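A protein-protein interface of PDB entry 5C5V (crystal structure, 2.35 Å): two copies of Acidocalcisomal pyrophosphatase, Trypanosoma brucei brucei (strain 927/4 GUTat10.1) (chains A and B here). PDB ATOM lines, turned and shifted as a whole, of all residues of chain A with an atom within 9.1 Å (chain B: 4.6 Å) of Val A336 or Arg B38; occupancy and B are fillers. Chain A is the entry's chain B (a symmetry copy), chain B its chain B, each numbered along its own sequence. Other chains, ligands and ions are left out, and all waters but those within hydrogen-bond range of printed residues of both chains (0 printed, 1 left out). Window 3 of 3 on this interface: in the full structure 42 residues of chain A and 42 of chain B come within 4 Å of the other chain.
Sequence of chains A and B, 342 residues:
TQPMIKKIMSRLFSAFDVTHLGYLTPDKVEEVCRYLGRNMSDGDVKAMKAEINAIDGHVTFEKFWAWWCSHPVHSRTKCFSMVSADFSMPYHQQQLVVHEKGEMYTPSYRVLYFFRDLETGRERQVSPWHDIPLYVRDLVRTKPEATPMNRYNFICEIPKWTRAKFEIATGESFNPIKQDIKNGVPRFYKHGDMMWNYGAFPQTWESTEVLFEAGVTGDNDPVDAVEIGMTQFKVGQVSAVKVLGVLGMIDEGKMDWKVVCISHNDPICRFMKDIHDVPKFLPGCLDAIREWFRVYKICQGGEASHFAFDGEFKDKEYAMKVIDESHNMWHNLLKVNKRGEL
The backbone carbonyl oxygen (O) of Ala B15 sits close to the side-chain amide oxygen (OD1) of Asn A332, 3.1 Å away.
No position is printed for both chains.
Printed residues of chain B within 4 Å of Asn A328: Ala B15.
Of the printed residues of chain B, Asn A332 touches Ala B15 and Phe B16.
Of chain B, only Phe B16 (3.6 Å), Tyr B35 (3.7 Å) and Arg B38 (3.6 Å) come within 4 Å of Val A336.
Of the printed residues of chain B, Lys A338 touches Arg B38.
Of the printed residues of chain A, Ala B15 touches Asn A328, His A331 and Asn A332.
No residue of chain A comes within 4 Å of Gly B37.
Asn B39 touches none of the printed residues of chain A.
The nearest residue of chain B that does not touch Val A336 is Phe B87 (4.3 Å).
The nearest printed residue of chain B that does not touch Asn A332 is Phe B87 (5.8 Å).
Of the 12 printed residues of chain A, 6 touch a printed residue of chain B.
Hydrophobic or aromatic side chains of chain A within 4 Å of the printed part of chain B: His A331 and Val A336.
Of the 11 printed residues of chain B, 5 touch a printed residue of chain A.
Printed residues of chain B that touch a printed residue of chain A: Ala B15, Phe B16, Tyr B35, Arg B38 and Phe B87.
Hydrophobic or aromatic side chains of chain B that line the printed part of chain A: Ala B15, Phe B16, Tyr B35 and Phe B87.
Among the printed residues, no Asp or Glu carboxylate lies within 4 Å of a Lys or Arg side-chain nitrogen of the other chain.
O of Asn A328 touches CA of Ala B15, 3.9 Å away.
CB of His A331 touches CB of Ala B15, 3.9 Å away.
His A331 touches Phe B87 (CD2 to CE1, 3.5 Å).
Asn A332 touches Phe B16 (OD1 to CE1, 3.9 Å).
Arg B38 touches Lys A335 (NH2 to O, 3.7 Å).
Val A336 touches Phe B16 (CG1 to CZ, 3.6 Å).
Val A336 touches Tyr B35.
Val A336 touches Arg B38.
NH2 of Arg B38 touches CE of Lys A338 (3.0 Å).
The backbone carbonyl oxygen of His A331 lies within hydrogen-bond range of the backbone NH of Val A336.
The side-chain amide nitrogen of Asn A332 lies close to the side-chain amide nitrogen of Asn A337 (2.9 Å).
The backbone NH of Lys A338 is in hydrogen-bond range of the backbone carbonyl oxygen of Leu A333 (3.3 Å).
The side-chain amino group of Lys A338 is in hydrogen-bond range of the backbone carbonyl oxygen of Lys A335 (3.1 Å).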
ATOM      1  N   ASN A 328     -22.162  20.476 -16.237  1.00  0.00           N
ATOM      2  CA  ASN A 328     -22.253  19.729 -17.496  1.00  0.00           C
ATOM      3  C   ASN A 328     -23.219  18.554 -17.371  1.00  0.00           C
ATOM      4  O   ASN A 328     -24.039  18.327 -18.254  1.00  0.00           O
ATOM      5  CB  ASN A 328     -20.874  19.219 -17.939  1.00  0.00           C
ATOM      6  CG  ASN A 328     -19.936  20.341 -18.355  1.00  0.00           C
ATOM      7  OD1 ASN A 328     -20.367  21.400 -18.781  1.00  0.00           O
ATOM      8  ND2 ASN A 328     -18.642  20.107 -18.228  1.00  0.00           N
ATOM      9  N   MET A 329     -23.112  17.820 -16.267  1.00  0.00           N
ATOM     10  CA  MET A 329     -23.988  16.686 -15.986  1.00  0.00           C
ATOM     11  C   MET A 329     -25.430  17.134 -15.895  1.00  0.00           C
ATOM     12  O   MET A 329     -26.332  16.446 -16.367  1.00  0.00           O
ATOM     13  CB  MET A 329     -23.602  15.988 -14.670  1.00  0.00           C
ATOM     14  CG  MET A 329     -22.215  15.377 -14.650  1.00  0.00           C
ATOM     15  SD  MET A 329     -21.631  14.993 -12.967  1.00  0.00           S
ATOM     16  CE  MET A 329     -19.938  14.568 -13.356  1.00  0.00           C
ATOM     17  N   TRP A 330     -25.645  18.281 -15.266  1.00  0.00           N
ATOM     18  CA  TRP A 330     -26.978  18.831 -15.159  1.00  0.00           C
ATOM     19  C   TRP A 330     -27.515  19.213 -16.540  1.00  0.00           C
ATOM     20  O   TRP A 330     -28.697  19.031 -16.814  1.00  0.00           O
ATOM     21  CB  TRP A 330     -26.989  20.038 -14.216  1.00  0.00           C
ATOM     22  CG  TRP A 330     -28.259  20.828 -14.298  1.00  0.00           C
ATOM     23  CD1 TRP A 330     -29.434  20.575 -13.647  1.00  0.00           C
ATOM     24  CD2 TRP A 330     -28.483  21.996 -15.090  1.00  0.00           C
ATOM     25  NE1 TRP A 330     -30.372  21.524 -13.973  1.00  0.00           N
ATOM     26  CE2 TRP A 330     -29.817  22.409 -14.859  1.00  0.00           C
ATOM     27  CE3 TRP A 330     -27.687  22.739 -15.964  1.00  0.00           C
ATOM     28  CZ2 TRP A 330     -30.372  23.526 -15.479  1.00  0.00           C
ATOM     29  CZ3 TRP A 330     -28.239  23.855 -16.572  1.00  0.00           C
ATOM     30  CH2 TRP A 330     -29.569  24.237 -16.323  1.00  0.00           C
ATOM     31  N   HIS A 331     -26.652  19.739 -17.406  1.00  0.00           N
ATOM     32  CA  HIS A 331     -27.064  20.045 -18.777  1.00  0.00           C
ATOM     33  C   HIS A 331     -27.528  18.776 -19.493  1.00  0.00           C
ATOM     34  O   HIS A 331     -28.535  18.789 -20.188  1.00  0.00           O
ATOM     35  CB  HIS A 331     -25.935  20.696 -19.573  1.00  0.00           C
ATOM     36  CG  HIS A 331     -25.885  22.183 -19.453  1.00  0.00           C
ATOM     37  ND1 HIS A 331     -25.090  22.831 -18.530  1.00  0.00           N
ATOM     38  CD2 HIS A 331     -26.517  23.155 -20.151  1.00  0.00           C
ATOM     39  CE1 HIS A 331     -25.245  24.135 -18.659  1.00  0.00           C
ATOM     40  NE2 HIS A 331     -26.106  24.359 -19.637  1.00  0.00           N
ATOM     41  N   ASN A 332     -26.795  17.683 -19.314  1.00  0.00           N
ATOM     42  CA  ASN A 332     -27.173  16.425 -19.943  1.00  0.00           C
ATOM     43  C   ASN A 332     -28.484  15.919 -19.359  1.00  0.00           C
ATOM     44  O   ASN A 332     -29.329  15.403 -20.087  1.00  0.00           O
ATOM     45  CB  ASN A 332     -26.074  15.360 -19.785  1.00  0.00           C
ATOM     46  CG  ASN A 332     -26.365  14.093 -20.591  1.00  0.00           C
ATOM     47  OD1 ASN A 332     -25.997  13.988 -21.760  1.00  0.00           O
ATOM     48  ND2 ASN A 332     -27.032  13.133 -19.966  1.00  0.00           N
ATOM     49  N   LEU A 333     -28.659  16.087 -18.050  1.00  0.00           N
ATOM     50  CA  LEU A 333     -29.875  15.620 -17.389  1.00  0.00           C
ATOM     51  C   LEU A 333     -31.103  16.392 -17.857  1.00  0.00           C
ATOM     52  O   LEU A 333     -32.090  15.798 -18.309  1.00  0.00           O
ATOM     53  CB  LEU A 333     -29.754  15.736 -15.877  1.00  0.00           C
ATOM     54  CG  LEU A 333     -31.021  15.455 -15.068  1.00  0.00           C
ATOM     55  CD1 LEU A 333     -31.270  13.974 -14.894  1.00  0.00           C
ATOM     56  CD2 LEU A 333     -30.896  16.136 -13.730  1.00  0.00           C
ATOM     57  N   LEU A 334     -31.036  17.718 -17.768  1.00  0.00           N
ATOM     58  CA  LEU A 334     -32.208  18.540 -18.032  1.00  0.00           C
ATOM     59  C   LEU A 334     -32.407  18.845 -19.513  1.00  0.00           C
ATOM     60  O   LEU A 334     -33.451  18.522 -20.075  1.00  0.00           O
ATOM     61  CB  LEU A 334     -32.121  19.853 -17.256  1.00  0.00           C
ATOM     62  CG  LEU A 334     -33.357  20.727 -17.442  1.00  0.00           C
ATOM     63  CD1 LEU A 334     -34.579  19.992 -16.913  1.00  0.00           C
ATOM     64  CD2 LEU A 334     -33.192  22.032 -16.731  1.00  0.00           C
ATOM     65  N   LYS A 335     -31.404  19.435 -20.157  1.00  0.00           N
ATOM     66  CA  LYS A 335     -31.551  19.854 -21.551  1.00  0.00           C
ATOM     67  C   LYS A 335     -31.618  18.667 -22.507  1.00  0.00           C
ATOM     68  O   LYS A 335     -32.548  18.546 -23.302  1.00  0.00           O
ATOM     69  CB  LYS A 335     -30.397  20.770 -21.967  1.00  0.00           C
ATOM     70  CG  LYS A 335     -30.094  21.921 -21.027  1.00  0.00           C
ATOM     71  CD  LYS A 335     -31.249  22.902 -20.928  1.00  0.00           C
ATOM     72  CE  LYS A 335     -30.808  24.171 -20.201  1.00  0.00           C
ATOM     73  NZ  LYS A 335     -31.916  25.164 -20.051  1.00  0.00           N
ATOM     74  N   VAL A 336     -30.632  17.783 -22.429  1.00  0.00           N
ATOM     75  CA  VAL A 336     -30.559  16.665 -23.357  1.00  0.00           C
ATOM     76  C   VAL A 336     -31.594  15.582 -23.070  1.00  0.00           C
ATOM     77  O   VAL A 336     -32.223  15.076 -23.988  1.00  0.00           O
ATOM     78  CB  VAL A 336     -29.170  16.032 -23.358  1.00  0.00           C
ATOM     79  CG1 VAL A 336     -29.125  14.868 -24.351  1.00  0.00           C
ATOM     80  CG2 VAL A 336     -28.126  17.081 -23.702  1.00  0.00           C
ATOM     81  N   ASN A 337     -31.751  15.183 -21.816  1.00  0.00           N
ATOM     82  CA  ASN A 337     -32.667  14.085 -21.523  1.00  0.00           C
ATOM     83  C   ASN A 337     -34.009  14.507 -20.924  1.00  0.00           C
ATOM     84  O   ASN A 337     -34.814  13.648 -20.564  1.00  0.00           O
ATOM     85  CB  ASN A 337     -31.997  13.070 -20.604  1.00  0.00           C
ATOM     86  CG  ASN A 337     -30.919  12.278 -21.313  1.00  0.00           C
ATOM     87  OD1 ASN A 337     -31.200  11.528 -22.251  1.00  0.00           O
ATOM     88  ND2 ASN A 337     -29.681  12.426 -20.865  1.00  0.00           N
ATOM     89  N   LYS A 338     -34.239  15.814 -20.813  1.00  0.00           N
ATOM     90  CA  LYS A 338     -35.532  16.349 -20.371  1.00  0.00           C
ATOM     91  C   LYS A 338     -36.000  15.851 -19.005  1.00  0.00           C
ATOM     92  O   LYS A 338     -37.202  15.765 -18.756  1.00  0.00           O
ATOM     93  CB  LYS A 338     -36.622  16.034 -21.407  1.00  0.00           C
ATOM     94  CG  LYS A 338     -36.298  16.505 -22.817  1.00  0.00           C
ATOM     95  CD  LYS A 338     -36.025  18.005 -22.788  1.00  0.00           C
ATOM     96  CE  LYS A 338     -35.697  18.583 -24.168  1.00  0.00           C
ATOM     97  NZ  LYS A 338     -35.232  20.008 -23.977  1.00  0.00           N
ATOM     98  N   ARG A 339     -35.072  15.549 -18.106  1.00  0.00           N
ATOM     99  CA  ARG A 339     -35.464  15.102 -16.772  1.00  0.00           C
ATOM    100  C   ARG A 339     -35.431  16.264 -15.791  1.00  0.00           C
ATOM    101  O   ARG A 339     -34.364  16.673 -15.347  1.00  0.00           O
ATOM    102  CB  ARG A 339     -34.552  13.959 -16.301  1.00  0.00           C
ATOM    103  CG  ARG A 339     -34.696  12.689 -17.154  1.00  0.00           C
ATOM    104  CD  ARG A 339     -33.630  11.632 -16.873  1.00  0.00           C
ATOM    105  NE  ARG A 339     -33.670  11.127 -15.505  1.00  0.00           N
ATOM    106  CZ  ARG A 339     -32.673  10.443 -14.942  1.00  0.00           C
ATOM    107  NH1 ARG A 339     -31.574  10.183 -15.643  1.00  0.00           N
ATOM    108  NH2 ARG A 339     -32.766  10.028 -13.678  1.00  0.00           N
ATOM    109  N   ALA B  15     -21.686  18.805 -22.560  1.00  0.00           N
ATOM    110  CA  ALA B  15     -22.791  18.078 -21.955  1.00  0.00           C
ATOM    111  C   ALA B  15     -22.730  16.595 -22.292  1.00  0.00           C
ATOM    112  O   ALA B  15     -23.507  15.810 -21.759  1.00  0.00           O
ATOM    113  CB  ALA B  15     -24.115  18.669 -22.388  1.00  0.00           C
ATOM    114  N   PHE B  16     -21.814  16.214 -23.181  1.00  0.00           N
ATOM    115  CA  PHE B  16     -21.612  14.808 -23.522  1.00  0.00           C
ATOM    116  C   PHE B  16     -20.205  14.326 -23.179  1.00  0.00           C
ATOM    117  O   PHE B  16     -19.884  13.158 -23.337  1.00  0.00           O
ATOM    118  CB  PHE B  16     -21.889  14.578 -25.008  1.00  0.00           C
ATOM    119  CG  PHE B  16     -23.318  14.803 -25.392  1.00  0.00           C
ATOM    120  CD1 PHE B  16     -24.244  13.781 -25.292  1.00  0.00           C
ATOM    121  CD2 PHE B  16     -23.742  16.046 -25.831  1.00  0.00           C
ATOM    122  CE1 PHE B  16     -25.561  13.986 -25.632  1.00  0.00           C
ATOM    123  CE2 PHE B  16     -25.064  16.251 -26.183  1.00  0.00           C
ATOM    124  CZ  PHE B  16     -25.971  15.218 -26.079  1.00  0.00           C
ATOM    125  N   ARG B  34     -28.481  10.948 -31.252  1.00  0.00           N
ATOM    126  CA  ARG B  34     -29.836  10.795 -30.763  1.00  0.00           C
ATOM    127  C   ARG B  34     -30.374  12.147 -30.255  1.00  0.00           C
ATOM    128  O   ARG B  34     -31.569  12.417 -30.323  1.00  0.00           O
ATOM    129  CB  ARG B  34     -29.865   9.721 -29.671  1.00  0.00           C
ATOM    130  CG  ARG B  34     -31.067   9.741 -28.745  1.00  0.00           C
ATOM    131  CD  ARG B  34     -31.002   8.569 -27.768  1.00  0.00           C
ATOM    132  NE  ARG B  34     -30.536   7.346 -28.426  1.00  0.00           N
ATOM    133  CZ  ARG B  34     -29.404   6.720 -28.111  1.00  0.00           C
ATOM    134  NH1 ARG B  34     -29.046   5.617 -28.759  1.00  0.00           N
ATOM    135  NH2 ARG B  34     -28.633   7.194 -27.133  1.00  0.00           N
ATOM    136  N   TYR B  35     -29.493  13.003 -29.756  1.00  0.00           N
ATOM    137  CA  TYR B  35     -29.931  14.314 -29.266  1.00  0.00           C
ATOM    138  C   TYR B  35     -30.138  15.268 -30.443  1.00  0.00           C
ATOM    139  O   TYR B  35     -31.200  15.870 -30.589  1.00  0.00           O
ATOM    140  CB  TYR B  35     -28.931  14.912 -28.261  1.00  0.00           C
ATOM    141  CG  TYR B  35     -29.175  16.387 -28.002  1.00  0.00           C
ATOM    142  CD1 TYR B  35     -30.289  16.815 -27.290  1.00  0.00           C
ATOM    143  CD2 TYR B  35     -28.299  17.349 -28.482  1.00  0.00           C
ATOM    144  CE1 TYR B  35     -30.526  18.161 -27.073  1.00  0.00           C
ATOM    145  CE2 TYR B  35     -28.524  18.694 -28.264  1.00  0.00           C
ATOM    146  CZ  TYR B  35     -29.639  19.093 -27.561  1.00  0.00           C
ATOM    147  OH  TYR B  35     -29.861  20.432 -27.343  1.00  0.00           O
ATOM    148  N   LEU B  36     -29.118  15.394 -31.283  1.00  0.00           N
ATOM    149  CA  LEU B  36     -29.199  16.246 -32.451  1.00  0.00           C
ATOM    150  C   LEU B  36     -30.286  15.754 -33.376  1.00  0.00           C
ATOM    151  O   LEU B  36     -30.917  16.545 -34.064  1.00  0.00           O
ATOM    152  CB  LEU B  36     -27.863  16.299 -33.198  1.00  0.00           C
ATOM    153  CG  LEU B  36     -26.762  17.117 -32.522  1.00  0.00           C
ATOM    154  CD1 LEU B  36     -25.476  17.012 -33.315  1.00  0.00           C
ATOM    155  CD2 LEU B  36     -27.197  18.564 -32.386  1.00  0.00           C
ATOM    156  N   GLY B  37     -30.513  14.443 -33.381  1.00  0.00           N
ATOM    157  CA  GLY B  37     -31.439  13.855 -34.324  1.00  0.00           C
ATOM    158  C   GLY B  37     -32.916  13.897 -34.017  1.00  0.00           C
ATOM    159  O   GLY B  37     -33.718  13.589 -34.882  1.00  0.00           O
ATOM    160  N   ARG B  38     -33.314  14.219 -32.797  1.00  0.00           N
ATOM    161  CA  ARG B  38     -34.737  14.458 -32.602  1.00  0.00           C
ATOM    162  C   ARG B  38     -35.009  15.845 -33.191  1.00  0.00           C
ATOM    163  O   ARG B  38     -34.258  16.791 -32.929  1.00  0.00           O
ATOM    164  CB  ARG B  38     -35.179  14.359 -31.129  1.00  0.00           C
ATOM    165  CG  ARG B  38     -35.348  15.689 -30.384  1.00  0.00           C
ATOM    166  CD  ARG B  38     -35.964  15.461 -29.009  1.00  0.00           C
ATOM    167  NE  ARG B  38     -35.492  16.396 -27.992  1.00  0.00           N
ATOM    168  CZ  ARG B  38     -34.529  16.127 -27.117  1.00  0.00           C
ATOM    169  NH1 ARG B  38     -33.950  14.928 -27.112  1.00  0.00           N
ATOM    170  NH2 ARG B  38     -34.173  17.042 -26.221  1.00  0.00           N
ATOM    171  N   ASN B  39     -36.045  15.975 -34.004  1.00  0.00           N
ATOM    172  CA  ASN B  39     -36.766  14.847 -34.525  1.00  0.00           C
ATOM    173  C   ASN B  39     -36.439  14.708 -36.009  1.00  0.00           C
ATOM    174  O   ASN B  39     -36.946  15.468 -36.839  1.00  0.00           O
ATOM    175  CB  ASN B  39     -38.271  15.022 -34.304  1.00  0.00           C
ATOM    176  N   MET B  40     -35.610  13.728 -36.345  1.00  0.00           N
ATOM    177  CA  MET B  40     -35.210  13.514 -37.723  1.00  0.00           C
ATOM    178  C   MET B  40     -35.505  12.072 -38.040  1.00  0.00           C
ATOM    179  O   MET B  40     -35.893  11.315 -37.145  1.00  0.00           O
ATOM    180  CB  MET B  40     -33.718  13.795 -37.963  1.00  0.00           C
ATOM    181  CG  MET B  40     -33.155  15.118 -37.462  1.00  0.00           C
ATOM    182  SD  MET B  40     -31.413  15.236 -37.964  1.00  0.00           S
ATOM    183  CE  MET B  40     -30.969  16.872 -37.395  1.00  0.00           C
ATOM    184  N   MET B  82     -33.280  23.793 -31.684  1.00  0.00           N
ATOM    185  CA  MET B  82     -33.273  23.069 -30.425  1.00  0.00           C
ATOM    186  C   MET B  82     -31.978  23.347 -29.671  1.00  0.00           C
ATOM    187  O   MET B  82     -31.991  23.668 -28.487  1.00  0.00           O
ATOM    188  CB  MET B  82     -33.427  21.570 -30.674  1.00  0.00           C
ATOM    189  CG  MET B  82     -33.281  20.717 -29.425  1.00  0.00           C
ATOM    190  SD  MET B  82     -33.031  18.994 -29.876  1.00  0.00           S
ATOM    191  CE  MET B  82     -31.638  19.180 -30.984  1.00  0.00           C
ATOM    192  N   PHE B  87     -28.712  25.635 -25.302  1.00  0.00           N
ATOM    193  CA  PHE B  87     -27.318  25.946 -24.980  1.00  0.00           C
ATOM    194  C   PHE B  87     -26.860  27.368 -25.274  1.00  0.00           C
ATOM    195  O   PHE B  87     -25.702  27.701 -25.029  1.00  0.00           O
ATOM    196  CB  PHE B  87     -26.394  24.960 -25.703  1.00  0.00           C
ATOM    197  CG  PHE B  87     -26.418  23.584 -25.109  1.00  0.00           C
ATOM    198  CD1 PHE B  87     -25.662  23.287 -23.976  1.00  0.00           C
ATOM    199  CD2 PHE B  87     -27.215  22.595 -25.656  1.00  0.00           C
ATOM    200  CE1 PHE B  87     -25.697  22.033 -23.417  1.00  0.00           C
ATOM    201  CE2 PHE B  87     -27.249  21.334 -25.099  1.00  0.00           C
ATOM    202  CZ  PHE B  87     -26.490  21.054 -23.974  1.00  0.00           C
